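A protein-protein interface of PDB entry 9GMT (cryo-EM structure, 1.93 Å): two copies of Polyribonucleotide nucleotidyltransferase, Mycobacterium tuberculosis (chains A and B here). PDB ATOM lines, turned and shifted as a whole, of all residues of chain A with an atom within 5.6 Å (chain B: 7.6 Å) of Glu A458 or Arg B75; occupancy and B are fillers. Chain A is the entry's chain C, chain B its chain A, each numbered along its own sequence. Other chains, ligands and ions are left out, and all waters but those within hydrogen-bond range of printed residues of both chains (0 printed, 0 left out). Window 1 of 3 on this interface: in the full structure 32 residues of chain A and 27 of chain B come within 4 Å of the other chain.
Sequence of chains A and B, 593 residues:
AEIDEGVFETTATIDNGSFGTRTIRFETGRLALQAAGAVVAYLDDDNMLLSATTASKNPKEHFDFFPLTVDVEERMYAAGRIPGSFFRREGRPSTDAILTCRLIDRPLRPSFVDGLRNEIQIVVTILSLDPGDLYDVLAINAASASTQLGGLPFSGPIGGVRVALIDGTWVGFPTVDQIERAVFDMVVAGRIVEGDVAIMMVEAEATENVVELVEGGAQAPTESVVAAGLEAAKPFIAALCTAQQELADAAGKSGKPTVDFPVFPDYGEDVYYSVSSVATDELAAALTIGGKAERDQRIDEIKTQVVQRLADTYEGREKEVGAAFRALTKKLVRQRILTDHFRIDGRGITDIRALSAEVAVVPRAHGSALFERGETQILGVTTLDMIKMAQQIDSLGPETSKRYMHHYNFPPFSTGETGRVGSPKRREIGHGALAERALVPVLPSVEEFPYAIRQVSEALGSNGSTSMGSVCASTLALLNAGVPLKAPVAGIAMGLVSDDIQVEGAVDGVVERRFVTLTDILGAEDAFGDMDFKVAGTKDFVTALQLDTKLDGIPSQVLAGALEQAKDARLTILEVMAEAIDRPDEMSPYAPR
The side-chain carboxylate (OE1) of Glu B73 lies within salt-bridge range of the guanidinium group (NH1) of Arg B75. The backbone carbonyl oxygen of Leu A379 lies within hydrogen-bond range of the backbone NH of Glu A458 (3.0 Å). The backbone NH (N) of Asn A409 is in hydrogen-bond range of the backbone carbonyl oxygen (O) of Ser A457 (2.9 Å). ND2 of Asn A409 lies within hydrogen-bond range of OE2 of Glu A458 (3.4 Å). The backbone carbonyl oxygen (O) of Asn A409 lies within hydrogen-bond range of the backbone NH (N) of Ala A459, 3.0 Å away.
Of the 22 printed residues of chain B, 3 touch a printed residue of chain A. Hydrophobic or aromatic side chains of chain B within 4 Å of the printed part of chain A: Tyr B77. Among the printed residues, 5 pairs touch across the chains.
Printed residues of chain B within 4 Å of Asn A409: Arg B75 (3.6 Å) and Arg B89 (3.2 Å). Of the printed residues of chain B, Val A456 touches Tyr B77 (3.9 Å). Printed residues of chain B within 4 Å of Glu A458: Arg B75 (2.9 Å) and Tyr B77 (3.0 Å). Arg B75 touches just these residues of chain A: Asn A409 (3.6 Å) and Glu A458 (2.9 Å). Of the printed residues of chain A, Tyr B77 touches Val A456 (3.9 Å) and Glu A458 (3.0 Å). The nearest residue of chain A that does not touch Arg B75 is Val A456 (5.1 Å). The nearest printed residue of chain A that does not touch Arg B89 is Ser A457 (6.7 Å).
The guanidinium group of Arg B75 is in salt-bridge range of the side-chain carboxylate of Glu A458, at 2.9 Å. OE1 of Glu A458 is in hydrogen-bond range of OH of Tyr B77, 3.0 Å away. OD1 of Asn A409 is in hydrogen-bond range of NH2 of Arg B89 (3.2 Å).
Among the printed residues, merely in contact across the chains: Asn A409 with Arg B75 and Val A456 with Tyr B77.
No position is printed for both chains.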
ATOM      1  N   GLN A 377      15.629 -27.526  -1.685  1.00  0.00           N
ATOM      2  CA  GLN A 377      14.685 -28.603  -1.965  1.00  0.00           C
ATOM      3  C   GLN A 377      13.283 -28.027  -2.056  1.00  0.00           C
ATOM      4  O   GLN A 377      12.774 -27.491  -1.063  1.00  0.00           O
ATOM      5  CB  GLN A 377      14.750 -29.682  -0.884  1.00  0.00           C
ATOM      6  CG  GLN A 377      13.730 -30.784  -1.045  1.00  0.00           C
ATOM      7  CD  GLN A 377      13.809 -31.801   0.066  1.00  0.00           C
ATOM      8  OE1 GLN A 377      13.379 -31.543   1.184  1.00  0.00           O
ATOM      9  NE2 GLN A 377      14.365 -32.962  -0.233  1.00  0.00           N
ATOM     10  N   ILE A 378      12.661 -28.176  -3.230  1.00  0.00           N
ATOM     11  CA  ILE A 378      11.356 -27.605  -3.550  1.00  0.00           C
ATOM     12  C   ILE A 378      10.394 -28.728  -3.921  1.00  0.00           C
ATOM     13  O   ILE A 378      10.758 -29.643  -4.667  1.00  0.00           O
ATOM     14  CB  ILE A 378      11.445 -26.590  -4.706  1.00  0.00           C
ATOM     15  CG1 ILE A 378      12.515 -25.530  -4.442  1.00  0.00           C
ATOM     16  CG2 ILE A 378      10.091 -25.954  -4.960  1.00  0.00           C
ATOM     17  CD1 ILE A 378      12.179 -24.593  -3.322  1.00  0.00           C
ATOM     18  N   LEU A 379       9.170 -28.649  -3.404  1.00  0.00           N
ATOM     19  CA  LEU A 379       8.076 -29.552  -3.750  1.00  0.00           C
ATOM     20  C   LEU A 379       6.984 -28.764  -4.468  1.00  0.00           C
ATOM     21  O   LEU A 379       6.482 -27.773  -3.932  1.00  0.00           O
ATOM     22  CB  LEU A 379       7.509 -30.223  -2.499  1.00  0.00           C
ATOM     23  CG  LEU A 379       6.202 -31.002  -2.671  1.00  0.00           C
ATOM     24  CD1 LEU A 379       6.446 -32.307  -3.396  1.00  0.00           C
ATOM     25  CD2 LEU A 379       5.521 -31.246  -1.339  1.00  0.00           C
ATOM     26  N   GLY A 380       6.608 -29.207  -5.663  1.00  0.00           N
ATOM     27  CA  GLY A 380       5.593 -28.537  -6.469  1.00  0.00           C
ATOM     28  C   GLY A 380       4.379 -29.419  -6.703  1.00  0.00           C
ATOM     29  O   GLY A 380       4.518 -30.623  -6.925  1.00  0.00           O
ATOM     30  N   ASN A 409       5.273 -20.684  -0.765  1.00  0.00           N
ATOM     31  CA  ASN A 409       5.299 -20.745   0.692  1.00  0.00           C
ATOM     32  C   ASN A 409       6.707 -21.025   1.205  1.00  0.00           C
ATOM     33  O   ASN A 409       7.424 -21.877   0.664  1.00  0.00           O
ATOM     34  CB  ASN A 409       4.346 -21.817   1.226  1.00  0.00           C
ATOM     35  CG  ASN A 409       2.904 -21.567   0.843  1.00  0.00           C
ATOM     36  OD1 ASN A 409       2.311 -20.569   1.237  1.00  0.00           O
ATOM     37  ND2 ASN A 409       2.330 -22.478   0.078  1.00  0.00           N
ATOM     38  N   PRO A 411       8.181 -21.758   4.833  1.00  0.00           N
ATOM     39  CA  PRO A 411       7.982 -21.990   6.273  1.00  0.00           C
ATOM     40  C   PRO A 411       9.258 -21.767   7.064  1.00  0.00           C
ATOM     41  O   PRO A 411      10.364 -21.840   6.515  1.00  0.00           O
ATOM     42  CB  PRO A 411       7.546 -23.459   6.327  1.00  0.00           C
ATOM     43  CG  PRO A 411       8.210 -24.058   5.167  1.00  0.00           C
ATOM     44  CD  PRO A 411       8.163 -23.021   4.080  1.00  0.00           C
ATOM     45  N   VAL A 456       1.398 -24.598  -6.687  1.00  0.00           N
ATOM     46  CA  VAL A 456       1.879 -24.283  -5.348  1.00  0.00           C
ATOM     47  C   VAL A 456       3.314 -24.764  -5.204  1.00  0.00           C
ATOM     48  O   VAL A 456       3.654 -25.874  -5.624  1.00  0.00           O
ATOM     49  CB  VAL A 456       0.987 -24.906  -4.256  1.00  0.00           C
ATOM     50  CG1 VAL A 456       1.579 -24.653  -2.886  1.00  0.00           C
ATOM     51  CG2 VAL A 456      -0.418 -24.346  -4.328  1.00  0.00           C
ATOM     52  N   SER A 457       4.155 -23.920  -4.615  1.00  0.00           N
ATOM     53  CA  SER A 457       5.551 -24.236  -4.342  1.00  0.00           C
ATOM     54  C   SER A 457       5.786 -24.188  -2.840  1.00  0.00           C
ATOM     55  O   SER A 457       5.431 -23.201  -2.192  1.00  0.00           O
ATOM     56  CB  SER A 457       6.484 -23.252  -5.048  1.00  0.00           C
ATOM     57  OG  SER A 457       6.631 -23.569  -6.414  1.00  0.00           O
ATOM     58  N   GLU A 458       6.369 -25.248  -2.290  1.00  0.00           N
ATOM     59  CA  GLU A 458       6.716 -25.319  -0.874  1.00  0.00           C
ATOM     60  C   GLU A 458       8.230 -25.389  -0.754  1.00  0.00           C
ATOM     61  O   GLU A 458       8.844 -26.330  -1.263  1.00  0.00           O
ATOM     62  CB  GLU A 458       6.084 -26.540  -0.200  1.00  0.00           C
ATOM     63  CG  GLU A 458       4.634 -26.818  -0.565  1.00  0.00           C
ATOM     64  CD  GLU A 458       3.646 -26.087   0.320  1.00  0.00           C
ATOM     65  OE1 GLU A 458       2.441 -26.396   0.251  1.00  0.00           O
ATOM     66  OE2 GLU A 458       4.069 -25.208   1.092  1.00  0.00           O
ATOM     67  N   ALA A 459       8.832 -24.420  -0.070  1.00  0.00           N
ATOM     68  CA  ALA A 459      10.286 -24.440   0.092  1.00  0.00           C
ATOM     69  C   ALA A 459      10.632 -25.280   1.316  1.00  0.00           C
ATOM     70  O   ALA A 459      10.794 -24.771   2.421  1.00  0.00           O
ATOM     71  CB  ALA A 459      10.840 -23.027   0.206  1.00  0.00           C
ATOM     72  N   LEU A 460      10.752 -26.593   1.109  1.00  0.00           N
ATOM     73  CA  LEU A 460      11.063 -27.488   2.218  1.00  0.00           C
ATOM     74  C   LEU A 460      12.491 -27.305   2.717  1.00  0.00           C
ATOM     75  O   LEU A 460      12.751 -27.492   3.908  1.00  0.00           O
ATOM     76  CB  LEU A 460      10.815 -28.944   1.819  1.00  0.00           C
ATOM     77  CG  LEU A 460       9.372 -29.303   1.449  1.00  0.00           C
ATOM     78  CD1 LEU A 460       9.231 -30.784   1.172  1.00  0.00           C
ATOM     79  CD2 LEU A 460       8.411 -28.875   2.536  1.00  0.00           C
ATOM     80  N   GLY A 461      13.426 -26.955   1.845  1.00  0.00           N
ATOM     81  CA  GLY A 461      14.776 -26.640   2.280  1.00  0.00           C
ATOM     82  C   GLY A 461      15.352 -25.514   1.450  1.00  0.00           C
ATOM     83  O   GLY A 461      15.145 -25.450   0.241  1.00  0.00           O
ATOM     84  N   VAL B  72      -1.307 -26.554  12.344  1.00  0.00           N
ATOM     85  CA  VAL B  72      -1.803 -27.507  11.357  1.00  0.00           C
ATOM     86  C   VAL B  72      -2.156 -26.745  10.086  1.00  0.00           C
ATOM     87  O   VAL B  72      -2.948 -25.797  10.124  1.00  0.00           O
ATOM     88  CB  VAL B  72      -3.026 -28.281  11.882  1.00  0.00           C
ATOM     89  CG1 VAL B  72      -3.594 -29.172  10.797  1.00  0.00           C
ATOM     90  CG2 VAL B  72      -2.657 -29.094  13.104  1.00  0.00           C
ATOM     91  N   GLU B  73      -1.582 -27.170   8.963  1.00  0.00           N
ATOM     92  CA  GLU B  73      -1.739 -26.515   7.669  1.00  0.00           C
ATOM     93  C   GLU B  73      -2.472 -27.456   6.720  1.00  0.00           C
ATOM     94  O   GLU B  73      -1.891 -28.432   6.230  1.00  0.00           O
ATOM     95  CB  GLU B  73      -0.380 -26.118   7.100  1.00  0.00           C
ATOM     96  CG  GLU B  73       0.404 -25.169   7.982  1.00  0.00           C
ATOM     97  CD  GLU B  73      -0.024 -23.729   7.809  1.00  0.00           C
ATOM     98  OE1 GLU B  73       0.263 -23.148   6.743  1.00  0.00           O
ATOM     99  OE2 GLU B  73      -0.666 -23.181   8.728  1.00  0.00           O
ATOM    100  N   GLU B  74      -3.735 -27.147   6.447  1.00  0.00           N
ATOM    101  CA  GLU B  74      -4.539 -27.896   5.493  1.00  0.00           C
ATOM    102  C   GLU B  74      -4.352 -27.294   4.106  1.00  0.00           C
ATOM    103  O   GLU B  74      -4.537 -26.090   3.918  1.00  0.00           O
ATOM    104  CB  GLU B  74      -6.015 -27.863   5.885  1.00  0.00           C
ATOM    105  CG  GLU B  74      -6.335 -28.487   7.225  1.00  0.00           C
ATOM    106  CD  GLU B  74      -7.816 -28.423   7.551  1.00  0.00           C
ATOM    107  OE1 GLU B  74      -8.498 -27.519   7.036  1.00  0.00           O
ATOM    108  OE2 GLU B  74      -8.299 -29.269   8.327  1.00  0.00           O
ATOM    109  N   ARG B  75      -3.987 -28.126   3.140  1.00  0.00           N
ATOM    110  CA  ARG B  75      -3.843 -27.692   1.761  1.00  0.00           C
ATOM    111  C   ARG B  75      -5.005 -28.224   0.936  1.00  0.00           C
ATOM    112  O   ARG B  75      -5.318 -29.415   0.985  1.00  0.00           O
ATOM    113  CB  ARG B  75      -2.518 -28.171   1.169  1.00  0.00           C
ATOM    114  CG  ARG B  75      -1.276 -27.594   1.832  1.00  0.00           C
ATOM    115  CD  ARG B  75      -1.155 -26.099   1.605  1.00  0.00           C
ATOM    116  NE  ARG B  75       0.170 -25.601   1.951  1.00  0.00           N
ATOM    117  CZ  ARG B  75       0.419 -24.728   2.917  1.00  0.00           C
ATOM    118  NH1 ARG B  75      -0.549 -24.233   3.666  1.00  0.00           N
ATOM    119  NH2 ARG B  75       1.672 -24.349   3.141  1.00  0.00           N
ATOM    120  N   MET B  76      -5.651 -27.333   0.186  1.00  0.00           N
ATOM    121  CA  MET B  76      -6.789 -27.740  -0.628  1.00  0.00           C
ATOM    122  C   MET B  76      -6.405 -28.703  -1.742  1.00  0.00           C
ATOM    123  O   MET B  76      -7.243 -29.509  -2.154  1.00  0.00           O
ATOM    124  CB  MET B  76      -7.481 -26.519  -1.224  1.00  0.00           C
ATOM    125  CG  MET B  76      -8.637 -26.018  -0.407  1.00  0.00           C
ATOM    126  SD  MET B  76      -9.922 -27.255  -0.197  1.00  0.00           S
ATOM    127  CE  MET B  76     -10.721 -26.612   1.256  1.00  0.00           C
ATOM    128  N   TYR B  77      -5.161 -28.661  -2.227  1.00  0.00           N
ATOM    129  CA  TYR B  77      -4.762 -29.611  -3.261  1.00  0.00           C
ATOM    130  C   TYR B  77      -4.762 -31.049  -2.755  1.00  0.00           C
ATOM    131  O   TYR B  77      -4.758 -31.974  -3.569  1.00  0.00           O
ATOM    132  CB  TYR B  77      -3.397 -29.234  -3.865  1.00  0.00           C
ATOM    133  CG  TYR B  77      -2.187 -29.170  -2.941  1.00  0.00           C
ATOM    134  CD1 TYR B  77      -1.672 -30.305  -2.331  1.00  0.00           C
ATOM    135  CD2 TYR B  77      -1.533 -27.970  -2.721  1.00  0.00           C
ATOM    136  CE1 TYR B  77      -0.570 -30.239  -1.514  1.00  0.00           C
ATOM    137  CE2 TYR B  77      -0.427 -27.897  -1.908  1.00  0.00           C
ATOM    138  CZ  TYR B  77       0.049 -29.035  -1.307  1.00  0.00           C
ATOM    139  OH  TYR B  77       1.149 -28.971  -0.493  1.00  0.00           O
ATOM    140  N   ALA B  78      -4.766 -31.255  -1.435  1.00  0.00           N
ATOM    141  CA  ALA B  78      -4.925 -32.592  -0.876  1.00  0.00           C
ATOM    142  C   ALA B  78      -6.290 -33.191  -1.183  1.00  0.00           C
ATOM    143  O   ALA B  78      -6.451 -34.408  -1.074  1.00  0.00           O
ATOM    144  CB  ALA B  78      -4.701 -32.561   0.634  1.00  0.00           C
ATOM    145  N   ALA B  79      -7.274 -32.371  -1.549  1.00  0.00           N
ATOM    146  CA  ALA B  79      -8.572 -32.856  -1.987  1.00  0.00           C
ATOM    147  C   ALA B  79      -8.822 -32.640  -3.473  1.00  0.00           C
ATOM    148  O   ALA B  79      -9.943 -32.864  -3.932  1.00  0.00           O
ATOM    149  CB  ALA B  79      -9.688 -32.194  -1.174  1.00  0.00           C
ATOM    150  N   GLY B  80      -7.816 -32.218  -4.233  1.00  0.00           N
ATOM    151  CA  GLY B  80      -7.973 -31.997  -5.658  1.00  0.00           C
ATOM    152  C   GLY B  80      -8.936 -30.886  -6.019  1.00  0.00           C
ATOM    153  O   GLY B  80      -9.775 -31.057  -6.903  1.00  0.00           O
ATOM    154  N   ARG B  81      -8.809 -29.738  -5.359  1.00  0.00           N
ATOM    155  CA  ARG B  81      -9.776 -28.656  -5.469  1.00  0.00           C
ATOM    156  C   ARG B  81      -9.064 -27.318  -5.314  1.00  0.00           C
ATOM    157  O   ARG B  81      -8.056 -27.209  -4.615  1.00  0.00           O
ATOM    158  CB  ARG B  81     -10.859 -28.802  -4.397  1.00  0.00           C
ATOM    159  CG  ARG B  81     -12.229 -28.345  -4.778  1.00  0.00           C
ATOM    160  CD  ARG B  81     -13.253 -29.039  -3.904  1.00  0.00           C
ATOM    161  NE  ARG B  81     -13.443 -28.359  -2.630  1.00  0.00           N
ATOM    162  CZ  ARG B  81     -13.489 -28.974  -1.458  1.00  0.00           C
ATOM    163  NH1 ARG B  81     -13.328 -30.281  -1.357  1.00  0.00           N
ATOM    164  NH2 ARG B  81     -13.699 -28.259  -0.359  1.00  0.00           N
ATOM    165  N   PRO B  83      -9.318 -23.469  -3.817  1.00  0.00           N
ATOM    166  CA  PRO B  83     -10.080 -22.824  -2.738  1.00  0.00           C
ATOM    167  C   PRO B  83     -11.145 -21.878  -3.274  1.00  0.00           C
ATOM    168  O   PRO B  83     -10.955 -21.205  -4.287  1.00  0.00           O
ATOM    169  CB  PRO B  83      -9.008 -22.069  -1.946  1.00  0.00           C
ATOM    170  CG  PRO B  83      -7.730 -22.716  -2.305  1.00  0.00           C
ATOM    171  CD  PRO B  83      -7.872 -23.230  -3.697  1.00  0.00           C
ATOM    172  N   ARG B  89      -6.900 -18.532  -2.039  1.00  0.00           N
ATOM    173  CA  ARG B  89      -5.766 -18.992  -1.253  1.00  0.00           C
ATOM    174  C   ARG B  89      -6.245 -19.305   0.156  1.00  0.00           C
ATOM    175  O   ARG B  89      -7.205 -18.707   0.645  1.00  0.00           O
ATOM    176  CB  ARG B  89      -4.639 -17.946  -1.240  1.00  0.00           C
ATOM    177  CG  ARG B  89      -3.299 -18.452  -0.744  1.00  0.00           C
ATOM    178  CD  ARG B  89      -2.172 -17.480  -1.073  1.00  0.00           C
ATOM    179  NE  ARG B  89      -0.876 -17.982  -0.632  1.00  0.00           N
ATOM    180  CZ  ARG B  89       0.295 -17.512  -1.038  1.00  0.00           C
ATOM    181  NH1 ARG B  89       0.379 -16.522  -1.908  1.00  0.00           N
ATOM    182  NH2 ARG B  89       1.409 -18.056  -0.565  1.00  0.00           N
ATOM    183  N   GLU B  90      -5.577 -20.257   0.800  1.00  0.00           N
ATOM    184  CA  GLU B  90      -5.931 -20.624   2.164  1.00  0.00           C
ATOM    185  C   GLU B  90      -5.620 -19.479   3.119  1.00  0.00           C
ATOM    186  O   GLU B  90      -4.567 -18.846   3.027  1.00  0.00           O
ATOM    187  CB  GLU B  90      -5.176 -21.883   2.589  1.00  0.00           C
ATOM    188  CG  GLU B  90      -5.509 -23.122   1.776  1.00  0.00           C
ATOM    189  CD  GLU B  90      -4.573 -23.319   0.598  1.00  0.00           C
ATOM    190  OE1 GLU B  90      -3.739 -22.429   0.350  1.00  0.00           O
ATOM    191  OE2 GLU B  90      -4.675 -24.358  -0.079  1.00  0.00           O
ATOM    192  N   GLY B  91      -6.536 -19.220   4.047  1.00  0.00           N
ATOM    193  CA  GLY B  91      -6.368 -18.126   4.983  1.00  0.00           C
ATOM    194  C   GLY B  91      -6.218 -18.554   6.427  1.00  0.00           C
ATOM    195  O   GLY B  91      -5.324 -19.335   6.761  1.00  0.00           O
ATOM    196  N   VAL B 123       4.945 -28.158  13.271  1.00  0.00           N
ATOM    197  CA  VAL B 123       4.103 -27.821  12.127  1.00  0.00           C
ATOM    198  C   VAL B 123       3.754 -29.104  11.387  1.00  0.00           C
ATOM    199  O   VAL B 123       4.647 -29.872  11.019  1.00  0.00           O
ATOM    200  CB  VAL B 123       4.800 -26.828  11.178  1.00  0.00           C
ATOM    201  CG1 VAL B 123       3.887 -26.477  10.021  1.00  0.00           C
ATOM    202  CG2 VAL B 123       5.222 -25.582  11.919  1.00  0.00           C
ATOM    203  N   VAL B 124       2.463 -29.331  11.159  1.00  0.00           N
ATOM    204  CA  VAL B 124       1.985 -30.508  10.438  1.00  0.00           C
ATOM    205  C   VAL B 124       1.251 -30.048   9.187  1.00  0.00           C
ATOM    206  O   VAL B 124       0.286 -29.288   9.281  1.00  0.00           O
ATOM    207  CB  VAL B 124       1.060 -31.376  11.310  1.00  0.00           C
ATOM    208  CG1 VAL B 124       0.591 -32.586  10.528  1.00  0.00           C
ATOM    209  CG2 VAL B 124       1.764 -31.798  12.578  1.00  0.00           C
ATOM    210  N   THR B 125       1.684 -30.534   8.028  1.00  0.00           N
ATOM    211  CA  THR B 125       1.110 -30.160   6.739  1.00  0.00           C
ATOM    212  C   THR B 125       0.394 -31.352   6.118  1.00  0.00           C
ATOM    213  O   THR B 125       0.974 -32.434   6.011  1.00  0.00           O
ATOM    214  CB  THR B 125       2.200 -29.656   5.789  1.00  0.00           C
ATOM    215  OG1 THR B 125       2.959 -28.630   6.436  1.00  0.00           O
ATOM    216  CG2 THR B 125       1.590 -29.096   4.517  1.00  0.00           C
ATOM    217  N   ILE B 126      -0.853 -31.156   5.698  1.00  0.00           N
ATOM    218  CA  ILE B 126      -1.638 -32.232   5.096  1.00  0.00           C
ATOM    219  C   ILE B 126      -1.406 -32.229   3.590  1.00  0.00           C
ATOM    220  O   ILE B 126      -1.669 -31.230   2.917  1.00  0.00           O
ATOM    221  CB  ILE B 126      -3.131 -32.087   5.423  1.00  0.00           C
ATOM    222  CG1 ILE B 126      -3.334 -31.804   6.911  1.00  0.00           C
ATOM    223  CG2 ILE B 126      -3.885 -33.339   5.021  1.00  0.00           C
ATOM    224  CD1 ILE B 126      -2.839 -32.891   7.813  1.00  0.00           C
ATOM    225  N   LEU B 127      -0.930 -33.352   3.056  1.00  0.00           N
ATOM    226  CA  LEU B 127      -0.521 -33.438   1.657  1.00  0.00           C
ATOM    227  C   LEU B 127      -1.457 -34.250   0.777  1.00  0.00           C
ATOM    228  O   LEU B 127      -1.652 -33.890  -0.382  1.00  0.00           O
ATOM    229  CB  LEU B 127       0.896 -34.016   1.549  1.00  0.00           C
ATOM    230  CG  LEU B 127       2.012 -33.197   2.200  1.00  0.00           C
ATOM    231  CD1 LEU B 127       3.359 -33.878   2.051  1.00  0.00           C
ATOM    232  CD2 LEU B 127       2.062 -31.797   1.623  1.00  0.00           C
ATOM    233  N   SER B 128      -2.025 -35.351   1.268  1.00  0.00           N
ATOM    234  CA  SER B 128      -2.944 -36.139   0.453  1.00  0.00           C
ATOM    235  C   SER B 128      -3.974 -36.825   1.340  1.00  0.00           C
ATOM    236  O   SER B 128      -3.602 -37.446   2.337  1.00  0.00           O
ATOM    237  CB  SER B 128      -2.186 -37.179  -0.372  1.00  0.00           C
ATOM    238  OG  SER B 128      -3.058 -37.883  -1.224  1.00  0.00           O
ATOM    239  N   LEU B 129      -5.252 -36.738   0.961  1.00  0.00           N
ATOM    240  CA  LEU B 129      -6.346 -37.249   1.784  1.00  0.00           C
ATOM    241  C   LEU B 129      -7.364 -38.016   0.952  1.00  0.00           C
ATOM    242  O   LEU B 129      -7.908 -37.483  -0.016  1.00  0.00           O
ATOM    243  CB  LEU B 129      -7.049 -36.106   2.524  1.00  0.00           C
ATOM    244  CG  LEU B 129      -8.133 -36.500   3.528  1.00  0.00           C
ATOM    245  CD1 LEU B 129      -7.531 -37.252   4.700  1.00  0.00           C
ATOM    246  CD2 LEU B 129      -8.894 -35.283   4.007  1.00  0.00           C
ATOM    247  N   LEU B 396     -11.454 -29.106   4.158  1.00  0.00           N
ATOM    248  CA  LEU B 396     -10.815 -30.287   3.594  1.00  0.00           C
ATOM    249  C   LEU B 396     -11.551 -31.569   3.955  1.00  0.00           C
ATOM    250  O   LEU B 396     -11.533 -32.526   3.176  1.00  0.00           O
ATOM    251  CB  LEU B 396      -9.365 -30.348   4.072  1.00  0.00           C
ATOM    252  CG  LEU B 396      -8.394 -31.358   3.474  1.00  0.00           C
ATOM    253  CD1 LEU B 396      -8.309 -31.193   1.974  1.00  0.00           C
ATOM    254  CD2 LEU B 396      -7.035 -31.168   4.109  1.00  0.00           C
